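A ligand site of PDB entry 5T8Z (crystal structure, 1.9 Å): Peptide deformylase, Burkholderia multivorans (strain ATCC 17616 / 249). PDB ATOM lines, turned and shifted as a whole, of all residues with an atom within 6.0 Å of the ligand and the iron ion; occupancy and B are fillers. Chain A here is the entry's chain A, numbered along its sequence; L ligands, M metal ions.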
ATOM      1  N   ALA A  50      -6.942  24.840 -18.861  1.00  0.00           N
ATOM      2  CA  ALA A  50      -7.246  24.357 -17.521  1.00  0.00           C
ATOM      3  C   ALA A  50      -8.061  23.063 -17.522  1.00  0.00           C
ATOM      4  O   ALA A  50      -8.452  22.598 -16.438  1.00  0.00           O
ATOM      5  CB  ALA A  50      -7.968  25.443 -16.726  1.00  0.00           C
ATOM      6  N   ASN A  51      -8.315  22.474 -18.689  1.00  0.00           N
ATOM      7  CA  ASN A  51      -9.212  21.332 -18.853  1.00  0.00           C
ATOM      8  C   ASN A  51     -10.581  21.602 -18.227  1.00  0.00           C
ATOM      9  O   ASN A  51     -11.193  20.748 -17.582  1.00  0.00           O
ATOM     10  CB  ASN A  51      -8.595  20.045 -18.296  1.00  0.00           C
ATOM     11  N   GLY A  52     -11.083  22.822 -18.432  1.00  0.00           N
ATOM     12  CA  GLY A  52     -12.403  23.192 -17.940  1.00  0.00           C
ATOM     13  C   GLY A  52     -13.493  22.829 -18.922  1.00  0.00           C
ATOM     14  O   GLY A  52     -13.284  22.754 -20.129  1.00  0.00           O
ATOM     15  N   ALA A  53     -14.688  22.584 -18.385  1.00  0.00           N
ATOM     16  CA  ALA A  53     -15.852  22.286 -19.204  1.00  0.00           C
ATOM     17  C   ALA A  53     -16.667  23.533 -19.521  1.00  0.00           C
ATOM     18  O   ALA A  53     -17.537  23.474 -20.403  1.00  0.00           O
ATOM     19  CB  ALA A  53     -16.747  21.240 -18.543  1.00  0.00           C
ATOM     20  N   GLY A  54     -16.403  24.643 -18.839  1.00  0.00           N
ATOM     21  CA  GLY A  54     -17.026  25.924 -19.107  1.00  0.00           C
ATOM     22  C   GLY A  54     -16.175  27.038 -18.545  1.00  0.00           C
ATOM     23  O   GLY A  54     -15.211  26.799 -17.811  1.00  0.00           O
ATOM     24  N   LEU A  55     -16.518  28.275 -18.912  1.00  0.00           N
ATOM     25  CA  LEU A  55     -15.863  29.468 -18.388  1.00  0.00           C
ATOM     26  C   LEU A  55     -16.809  30.656 -18.542  1.00  0.00           C
ATOM     27  O   LEU A  55     -17.548  30.739 -19.524  1.00  0.00           O
ATOM     28  CB  LEU A  55     -14.532  29.751 -19.100  1.00  0.00           C
ATOM     29  CG  LEU A  55     -13.566  30.729 -18.408  1.00  0.00           C
ATOM     30  CD1 LEU A  55     -13.003  30.093 -17.128  1.00  0.00           C
ATOM     31  CD2 LEU A  55     -12.412  31.204 -19.293  1.00  0.00           C
ATOM     32  N   ALA A  56     -16.750  31.568 -17.585  1.00  0.00           N
ATOM     33  CA  ALA A  56     -17.542  32.794 -17.646  1.00  0.00           C
ATOM     34  C   ALA A  56     -16.618  34.006 -17.672  1.00  0.00           C
ATOM     35  O   ALA A  56     -15.573  34.007 -17.000  1.00  0.00           O
ATOM     36  CB  ALA A  56     -18.530  32.869 -16.442  1.00  0.00           C
ATOM     37  N   GLN A  59     -14.673  35.496 -14.688  1.00  0.00           N
ATOM     38  CA  GLN A  59     -13.534  34.737 -14.160  1.00  0.00           C
ATOM     39  C   GLN A  59     -12.207  35.187 -14.756  1.00  0.00           C
ATOM     40  O   GLN A  59     -11.151  34.902 -14.170  1.00  0.00           O
ATOM     41  CB  GLN A  59     -13.706  33.234 -14.416  1.00  0.00           C
ATOM     42  CG  GLN A  59     -14.907  32.574 -13.725  1.00  0.00           C
ATOM     43  CD  GLN A  59     -14.969  31.107 -14.041  1.00  0.00           C
ATOM     44  OE1 GLN A  59     -15.528  30.717 -15.082  1.00  0.00           O
ATOM     45  NE2 GLN A  59     -14.374  30.268 -13.183  1.00  0.00           N
ATOM     46  N   TRP A 104     -21.045  16.354  -7.799  1.00  0.00           N
ATOM     47  CA  TRP A 104     -19.776  16.992  -7.465  1.00  0.00           C
ATOM     48  C   TRP A 104     -19.452  18.092  -8.467  1.00  0.00           C
ATOM     49  O   TRP A 104     -19.559  17.878  -9.678  1.00  0.00           O
ATOM     50  CB  TRP A 104     -18.656  15.960  -7.478  1.00  0.00           C
ATOM     51  CG  TRP A 104     -18.754  15.004  -6.334  1.00  0.00           C
ATOM     52  CD1 TRP A 104     -19.274  13.739  -6.354  1.00  0.00           C
ATOM     53  CD2 TRP A 104     -18.352  15.253  -4.994  1.00  0.00           C
ATOM     54  NE1 TRP A 104     -19.193  13.172  -5.106  1.00  0.00           N
ATOM     55  CE2 TRP A 104     -18.622  14.087  -4.243  1.00  0.00           C
ATOM     56  CE3 TRP A 104     -17.759  16.348  -4.341  1.00  0.00           C
ATOM     57  CZ2 TRP A 104     -18.333  13.986  -2.892  1.00  0.00           C
ATOM     58  CZ3 TRP A 104     -17.482  16.248  -2.997  1.00  0.00           C
ATOM     59  CH2 TRP A 104     -17.767  15.071  -2.283  1.00  0.00           C
ATOM     60  N   GLU A 105     -19.056  19.270  -7.979  1.00  0.00           N
ATOM     61  CA  GLU A 105     -18.577  20.340  -8.834  1.00  0.00           C
ATOM     62  C   GLU A 105     -17.225  20.836  -8.337  1.00  0.00           C
ATOM     63  O   GLU A 105     -16.932  20.838  -7.136  1.00  0.00           O
ATOM     64  CB  GLU A 105     -19.555  21.515  -8.892  1.00  0.00           C
ATOM     65  CG  GLU A 105     -20.963  21.090  -9.296  1.00  0.00           C
ATOM     66  CD  GLU A 105     -21.897  22.259  -9.624  1.00  0.00           C
ATOM     67  OE1 GLU A 105     -21.459  23.427  -9.713  1.00  0.00           O
ATOM     68  OE2 GLU A 105     -23.108  21.984  -9.791  1.00  0.00           O
ATOM     69  N   GLY A 106     -16.378  21.239  -9.283  1.00  0.00           N
ATOM     70  CA  GLY A 106     -15.246  22.090  -9.019  1.00  0.00           C
ATOM     71  C   GLY A 106     -15.357  23.352  -9.859  1.00  0.00           C
ATOM     72  O   GLY A 106     -16.164  23.445 -10.796  1.00  0.00           O
ATOM     73  N   CYS A 107     -14.518  24.317  -9.525  1.00  0.00           N
ATOM     74  CA  CYS A 107     -14.511  25.626 -10.163  1.00  0.00           C
ATOM     75  C   CYS A 107     -13.067  26.050 -10.386  1.00  0.00           C
ATOM     76  O   CYS A 107     -12.237  25.914  -9.490  1.00  0.00           O
ATOM     77  CB  CYS A 107     -15.236  26.675  -9.303  1.00  0.00           C
ATOM     78  SG  CYS A 107     -15.440  28.301 -10.103  1.00  0.00           S
ATOM     79  N   LEU A 108     -12.783  26.572 -11.582  1.00  0.00           N
ATOM     80  CA  LEU A 108     -11.450  27.076 -11.841  1.00  0.00           C
ATOM     81  C   LEU A 108     -11.101  28.267 -10.945  1.00  0.00           C
ATOM     82  O   LEU A 108      -9.919  28.575 -10.779  1.00  0.00           O
ATOM     83  CB  LEU A 108     -11.321  27.451 -13.309  1.00  0.00           C
ATOM     84  CG  LEU A 108     -11.349  26.226 -14.222  1.00  0.00           C
ATOM     85  CD1 LEU A 108     -11.327  26.621 -15.696  1.00  0.00           C
ATOM     86  CD2 LEU A 108     -10.167  25.294 -13.877  1.00  0.00           C
ATOM     87  N   SER A 109     -12.103  28.921 -10.345  1.00  0.00           N
ATOM     88  CA  SER A 109     -11.877  29.996  -9.394  1.00  0.00           C
ATOM     89  C   SER A 109     -11.779  29.507  -7.941  1.00  0.00           C
ATOM     90  O   SER A 109     -11.529  30.306  -7.039  1.00  0.00           O
ATOM     91  CB  SER A 109     -13.017  31.035  -9.501  1.00  0.00           C
ATOM     92  OG  SER A 109     -13.000  31.661 -10.794  1.00  0.00           O
ATOM     93  N   MET A 113     -10.469  22.126  -4.972  1.00  0.00           N
ATOM     94  CA  MET A 113     -11.588  21.685  -4.152  1.00  0.00           C
ATOM     95  C   MET A 113     -12.721  21.111  -5.001  1.00  0.00           C
ATOM     96  O   MET A 113     -12.808  21.338  -6.212  1.00  0.00           O
ATOM     97  CB  MET A 113     -12.103  22.842  -3.303  1.00  0.00           C
ATOM     98  CG  MET A 113     -10.959  23.570  -2.597  1.00  0.00           C
ATOM     99  SD  MET A 113     -11.536  24.614  -1.279  1.00  0.00           S
ATOM    100  CE  MET A 113     -11.907  23.370  -0.027  1.00  0.00           C
ATOM    101  N   ARG A 114     -13.590  20.345  -4.330  1.00  0.00           N
ATOM    102  CA  ARG A 114     -14.853  19.857  -4.879  1.00  0.00           C
ATOM    103  C   ARG A 114     -15.937  19.947  -3.801  1.00  0.00           C
ATOM    104  O   ARG A 114     -15.651  19.829  -2.607  1.00  0.00           O
ATOM    105  CB  ARG A 114     -14.773  18.390  -5.340  1.00  0.00           C
ATOM    106  CG  ARG A 114     -13.701  18.102  -6.382  1.00  0.00           C
ATOM    107  CD  ARG A 114     -14.145  18.702  -7.736  1.00  0.00           C
ATOM    108  NE  ARG A 114     -13.270  18.261  -8.833  1.00  0.00           N
ATOM    109  CZ  ARG A 114     -12.240  18.959  -9.296  1.00  0.00           C
ATOM    110  NH1 ARG A 114     -11.929  20.138  -8.746  1.00  0.00           N
ATOM    111  NH2 ARG A 114     -11.511  18.486 -10.310  1.00  0.00           N
ATOM    112  N   PHE A 142     -25.737  16.757 -16.966  1.00  0.00           N
ATOM    113  CA  PHE A 142     -24.468  17.485 -16.877  1.00  0.00           C
ATOM    114  C   PHE A 142     -24.481  18.746 -17.740  1.00  0.00           C
ATOM    115  O   PHE A 142     -24.007  19.802 -17.322  1.00  0.00           O
ATOM    116  CB  PHE A 142     -23.304  16.561 -17.288  1.00  0.00           C
ATOM    117  CG  PHE A 142     -21.950  17.212 -17.143  1.00  0.00           C
ATOM    118  CD1 PHE A 142     -21.392  17.411 -15.888  1.00  0.00           C
ATOM    119  CD2 PHE A 142     -21.255  17.644 -18.259  1.00  0.00           C
ATOM    120  CE1 PHE A 142     -20.151  18.013 -15.745  1.00  0.00           C
ATOM    121  CE2 PHE A 142     -20.007  18.245 -18.128  1.00  0.00           C
ATOM    122  CZ  PHE A 142     -19.461  18.425 -16.870  1.00  0.00           C
ATOM    123  N   ARG A 145     -26.202  21.185 -15.779  1.00  0.00           N
ATOM    124  CA  ARG A 145     -25.382  21.563 -14.628  1.00  0.00           C
ATOM    125  C   ARG A 145     -24.329  22.594 -15.016  1.00  0.00           C
ATOM    126  O   ARG A 145     -24.162  23.623 -14.341  1.00  0.00           O
ATOM    127  CB  ARG A 145     -24.724  20.324 -14.033  1.00  0.00           C
ATOM    128  CG  ARG A 145     -23.764  20.639 -12.857  1.00  0.00           C
ATOM    129  CD  ARG A 145     -23.293  19.372 -12.175  1.00  0.00           C
ATOM    130  NE  ARG A 145     -24.418  18.628 -11.605  1.00  0.00           N
ATOM    131  CZ  ARG A 145     -24.864  18.750 -10.358  1.00  0.00           C
ATOM    132  NH1 ARG A 145     -24.279  19.583  -9.489  1.00  0.00           N
ATOM    133  NH2 ARG A 145     -25.907  17.999  -9.976  1.00  0.00           N
ATOM    134  N   VAL A 146     -23.590  22.338 -16.110  1.00  0.00           N
ATOM    135  CA  VAL A 146     -22.577  23.292 -16.526  1.00  0.00           C
ATOM    136  C   VAL A 146     -23.199  24.653 -16.785  1.00  0.00           C
ATOM    137  O   VAL A 146     -22.670  25.684 -16.353  1.00  0.00           O
ATOM    138  CB  VAL A 146     -21.828  22.797 -17.781  1.00  0.00           C
ATOM    139  CG1 VAL A 146     -20.879  23.874 -18.270  1.00  0.00           C
ATOM    140  CG2 VAL A 146     -21.048  21.542 -17.472  1.00  0.00           C
ATOM    141  N   HIS A 149     -23.979  26.387 -13.537  1.00  0.00           N
ATOM    142  CA  HIS A 149     -22.740  26.811 -12.883  1.00  0.00           C
ATOM    143  C   HIS A 149     -22.175  28.072 -13.526  1.00  0.00           C
ATOM    144  O   HIS A 149     -21.776  29.008 -12.825  1.00  0.00           O
ATOM    145  CB  HIS A 149     -21.767  25.660 -12.971  1.00  0.00           C
ATOM    146  CG  HIS A 149     -20.434  25.931 -12.360  1.00  0.00           C
ATOM    147  ND1 HIS A 149     -20.024  25.326 -11.195  1.00  0.00           N
ATOM    148  CD2 HIS A 149     -19.429  26.746 -12.750  1.00  0.00           C
ATOM    149  CE1 HIS A 149     -18.798  25.735 -10.908  1.00  0.00           C
ATOM    150  NE2 HIS A 149     -18.421  26.601 -11.831  1.00  0.00           N
ATOM    151  N   GLU A 150     -22.126  28.129 -14.868  1.00  0.00           N
ATOM    152  CA  GLU A 150     -21.572  29.311 -15.516  1.00  0.00           C
ATOM    153  C   GLU A 150     -22.502  30.500 -15.380  1.00  0.00           C
ATOM    154  O   GLU A 150     -22.032  31.637 -15.183  1.00  0.00           O
ATOM    155  CB  GLU A 150     -21.291  29.045 -17.001  1.00  0.00           C
ATOM    156  CG  GLU A 150     -20.379  27.853 -17.248  1.00  0.00           C
ATOM    157  CD  GLU A 150     -19.026  27.964 -16.557  1.00  0.00           C
ATOM    158  OE1 GLU A 150     -18.560  29.077 -16.242  1.00  0.00           O
ATOM    159  OE2 GLU A 150     -18.416  26.895 -16.339  1.00  0.00           O
ATOM    160  N   HIS A 153     -21.994  32.407 -12.257  1.00  0.00           N
ATOM    161  CA  HIS A 153     -20.874  33.357 -12.275  1.00  0.00           C
ATOM    162  C   HIS A 153     -21.314  34.741 -12.725  1.00  0.00           C
ATOM    163  O   HIS A 153     -20.713  35.733 -12.319  1.00  0.00           O
ATOM    164  CB  HIS A 153     -19.734  32.877 -13.180  1.00  0.00           C
ATOM    165  CG  HIS A 153     -18.824  31.917 -12.506  1.00  0.00           C
ATOM    166  ND1 HIS A 153     -18.110  32.245 -11.370  1.00  0.00           N
ATOM    167  CD2 HIS A 153     -18.500  30.633 -12.789  1.00  0.00           C
ATOM    168  CE1 HIS A 153     -17.380  31.210 -11.003  1.00  0.00           C
ATOM    169  NE2 HIS A 153     -17.609  30.220 -11.837  1.00  0.00           N
ATOM    170  N   TYR A 159     -19.984  28.270  -6.443  1.00  0.00           N
ATOM    171  CA  TYR A 159     -20.749  27.100  -6.006  1.00  0.00           C
ATOM    172  C   TYR A 159     -20.738  26.874  -4.493  1.00  0.00           C
ATOM    173  O   TYR A 159     -21.736  26.325  -3.991  1.00  0.00           O
ATOM    174  CB  TYR A 159     -20.309  25.833  -6.786  1.00  0.00           C
ATOM    175  CG  TYR A 159     -18.991  25.214  -6.311  1.00  0.00           C
ATOM    176  CD1 TYR A 159     -18.977  24.303  -5.260  1.00  0.00           C
ATOM    177  CD2 TYR A 159     -17.783  25.556  -6.907  1.00  0.00           C
ATOM    178  CE1 TYR A 159     -17.757  23.745  -4.782  1.00  0.00           C
ATOM    179  CE2 TYR A 159     -16.560  24.975  -6.473  1.00  0.00           C
ATOM    180  CZ  TYR A 159     -16.557  24.077  -5.396  1.00  0.00           C
ATOM    181  OH  TYR A 159     -15.359  23.529  -4.954  1.00  0.00           O
ATOM    182  N   PHE A 176     -10.937  12.485  -3.820  1.00  0.00           N
ATOM    183  CA  PHE A 176     -10.754  11.599  -4.979  1.00  0.00           C
ATOM    184  C   PHE A 176      -9.267  11.383  -5.255  1.00  0.00           C
ATOM    185  O   PHE A 176      -8.702  11.998  -6.167  1.00  0.00           O
ATOM    186  CB  PHE A 176     -11.447  12.180  -6.213  1.00  0.00           C
ATOM    187  CG  PHE A 176     -12.856  12.668  -5.988  1.00  0.00           C
ATOM    188  CD1 PHE A 176     -13.952  11.817  -6.180  1.00  0.00           C
ATOM    189  CD2 PHE A 176     -13.108  13.996  -5.667  1.00  0.00           C
ATOM    190  CE1 PHE A 176     -15.259  12.281  -6.022  1.00  0.00           C
ATOM    191  CE2 PHE A 176     -14.411  14.471  -5.500  1.00  0.00           C
ATOM    192  CZ  PHE A 176     -15.482  13.608  -5.679  1.00  0.00           C
HETATM  193  C1  LIG L   1     -15.129  25.135 -14.753  1.00  0.00           C
HETATM  194  C2  LIG L   1     -15.495  26.496 -14.191  1.00  0.00           C
HETATM  195  O1  LIG L   1     -14.979  26.930 -13.167  1.00  0.00           O
HETATM  196  N1  LIG L   1     -16.389  27.161 -14.900  1.00  0.00           N
HETATM  197  O2  LIG L   1     -16.927  28.345 -14.403  1.00  0.00           O
HETATM  198  C3  LIG L   1     -16.038  24.013 -14.257  1.00  0.00           C
HETATM  199  C4  LIG L   1     -15.369  22.685 -14.512  1.00  0.00           C
HETATM  200  O3  LIG L   1     -15.052  22.320 -15.648  1.00  0.00           O
HETATM  201  C5  LIG L   1     -17.347  24.063 -15.059  1.00  0.00           C
HETATM  202  C6  LIG L   1     -18.304  22.895 -14.810  1.00  0.00           C
HETATM  203  C7  LIG L   1     -18.964  22.923 -13.445  1.00  0.00           C
HETATM  204  C8  LIG L   1     -19.960  21.798 -13.225  1.00  0.00           C
HETATM  205  C9  LIG L   1     -19.318  20.437 -13.152  1.00  0.00           C
HETATM  206  N2  LIG L   1     -15.163  21.927 -13.423  1.00  0.00           N
HETATM  207  C10 LIG L   1     -14.637  20.579 -13.533  1.00  0.00           C
HETATM  208  C11 LIG L   1     -13.162  20.496 -13.096  1.00  0.00           C
HETATM  209  C12 LIG L   1     -12.235  20.955 -14.198  1.00  0.00           C
HETATM  210  C13 LIG L   1     -12.909  21.301 -11.824  1.00  0.00           C
HETATM  211  C14 LIG L   1     -15.548  19.621 -12.762  1.00  0.00           C
HETATM  212  O4  LIG L   1     -16.158  20.019 -11.777  1.00  0.00           O
HETATM  213  N3  LIG L   1     -15.678  18.366 -13.225  1.00  0.00           N
HETATM  214  C15 LIG L   1     -16.534  17.388 -12.536  1.00  0.00           C
HETATM  215  C16 LIG L   1     -15.055  17.806 -14.425  1.00  0.00           C
HETATM  216  C17 LIG L   1     -16.018  16.730 -14.831  1.00  0.00           C
HETATM  217  C18 LIG L   1     -16.568  16.202 -13.511  1.00  0.00           C
HETATM  218  C19 LIG L   1     -15.970  17.018 -11.162  1.00  0.00           C
HETATM  219  O5  LIG L   1     -16.685  15.941 -10.585  1.00  0.00           O
HETATM  220 FE    FE M   1     -16.740  28.087 -12.072  1.00  0.00          FE
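A nitrogen (N1) of the ligand is in hydrogen-bond range of the side-chain carboxylate (OE2) of Glu 150.
O1 of the ligand lies close to N of Leu 108.
N of Ala 53 sits at hydrogen-bond distance from O3 of the ligand.
O4 of the ligand is in hydrogen-bond range of N of Gly 106 (2.8 Å).
The backbone carbonyl oxygen of Gly 106 sits at hydrogen-bond distance from a nitrogen (N2) of the ligand (3.2 Å).
An oxygen (O2) of the ligand lies close to the side-chain amide oxygen of Gln 59.
The backbone carbonyl oxygen (O) of Gly 54 sits at hydrogen-bond distance from a nitrogen (N1) of the ligand (3.2 Å).
A ring nitrogen (ND1) of His 149 sits at hydrogen-bond distance from the side-chain carboxylate of Glu 105 (2.8 Å).
SG of Cys 107 sits close to N of Ser 109 (3.4 Å).
N of Leu 55 sits close to OE1 of Glu 150 (3.5 Å).
OE1 of Glu 150 is in hydrogen-bond range of N of Ala 56, at 3.4 Å.
NE2 of Gln 59 is in hydrogen-bond range of OG of Ser 109, 3.1 Å away.
The side-chain amide oxygen (OE1) of Gln 59 lies within hydrogen-bond range of the backbone NH (N) of Ala 56, at 2.9 Å.
The guanidinium group of Arg 145 lies within salt-bridge range of the side-chain carboxylate of Glu 105, at 2.7 Å.
Asn 51 touches the ligand.
Gly 52 touches the ligand.
Trp 104 touches the ligand (O to O5, 3.6 Å).
C of Glu 105 touches O4 of the ligand, at 3.7 Å.
Arg 114 touches the ligand.
Phe 142 touches the ligand (CE1 to C9, 3.6 Å).
Arg 145 touches the ligand.
Of the 24 residues printed, 16 come within 4 Å of the ligand.
The nearest printed residue that does not touch the ligand is Val 146 (4.1 Å).
Gln 59 touches the iron ion.
Four residues have an atom within 4 Å of the iron ion: Gln 59, Cys 107, His 149 and His 153.
The nearest printed residue that does not touch the iron ion is Leu 108 (4.3 Å).
The iron ion is bound by NE2 of His 149 (2.3 Å), NE2 of His 153 (2.3 Å), O2 of the ligand (2.4 Å), SG of Cys 107 (2.4 Å) and O1 of the ligand (2.4 Å).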
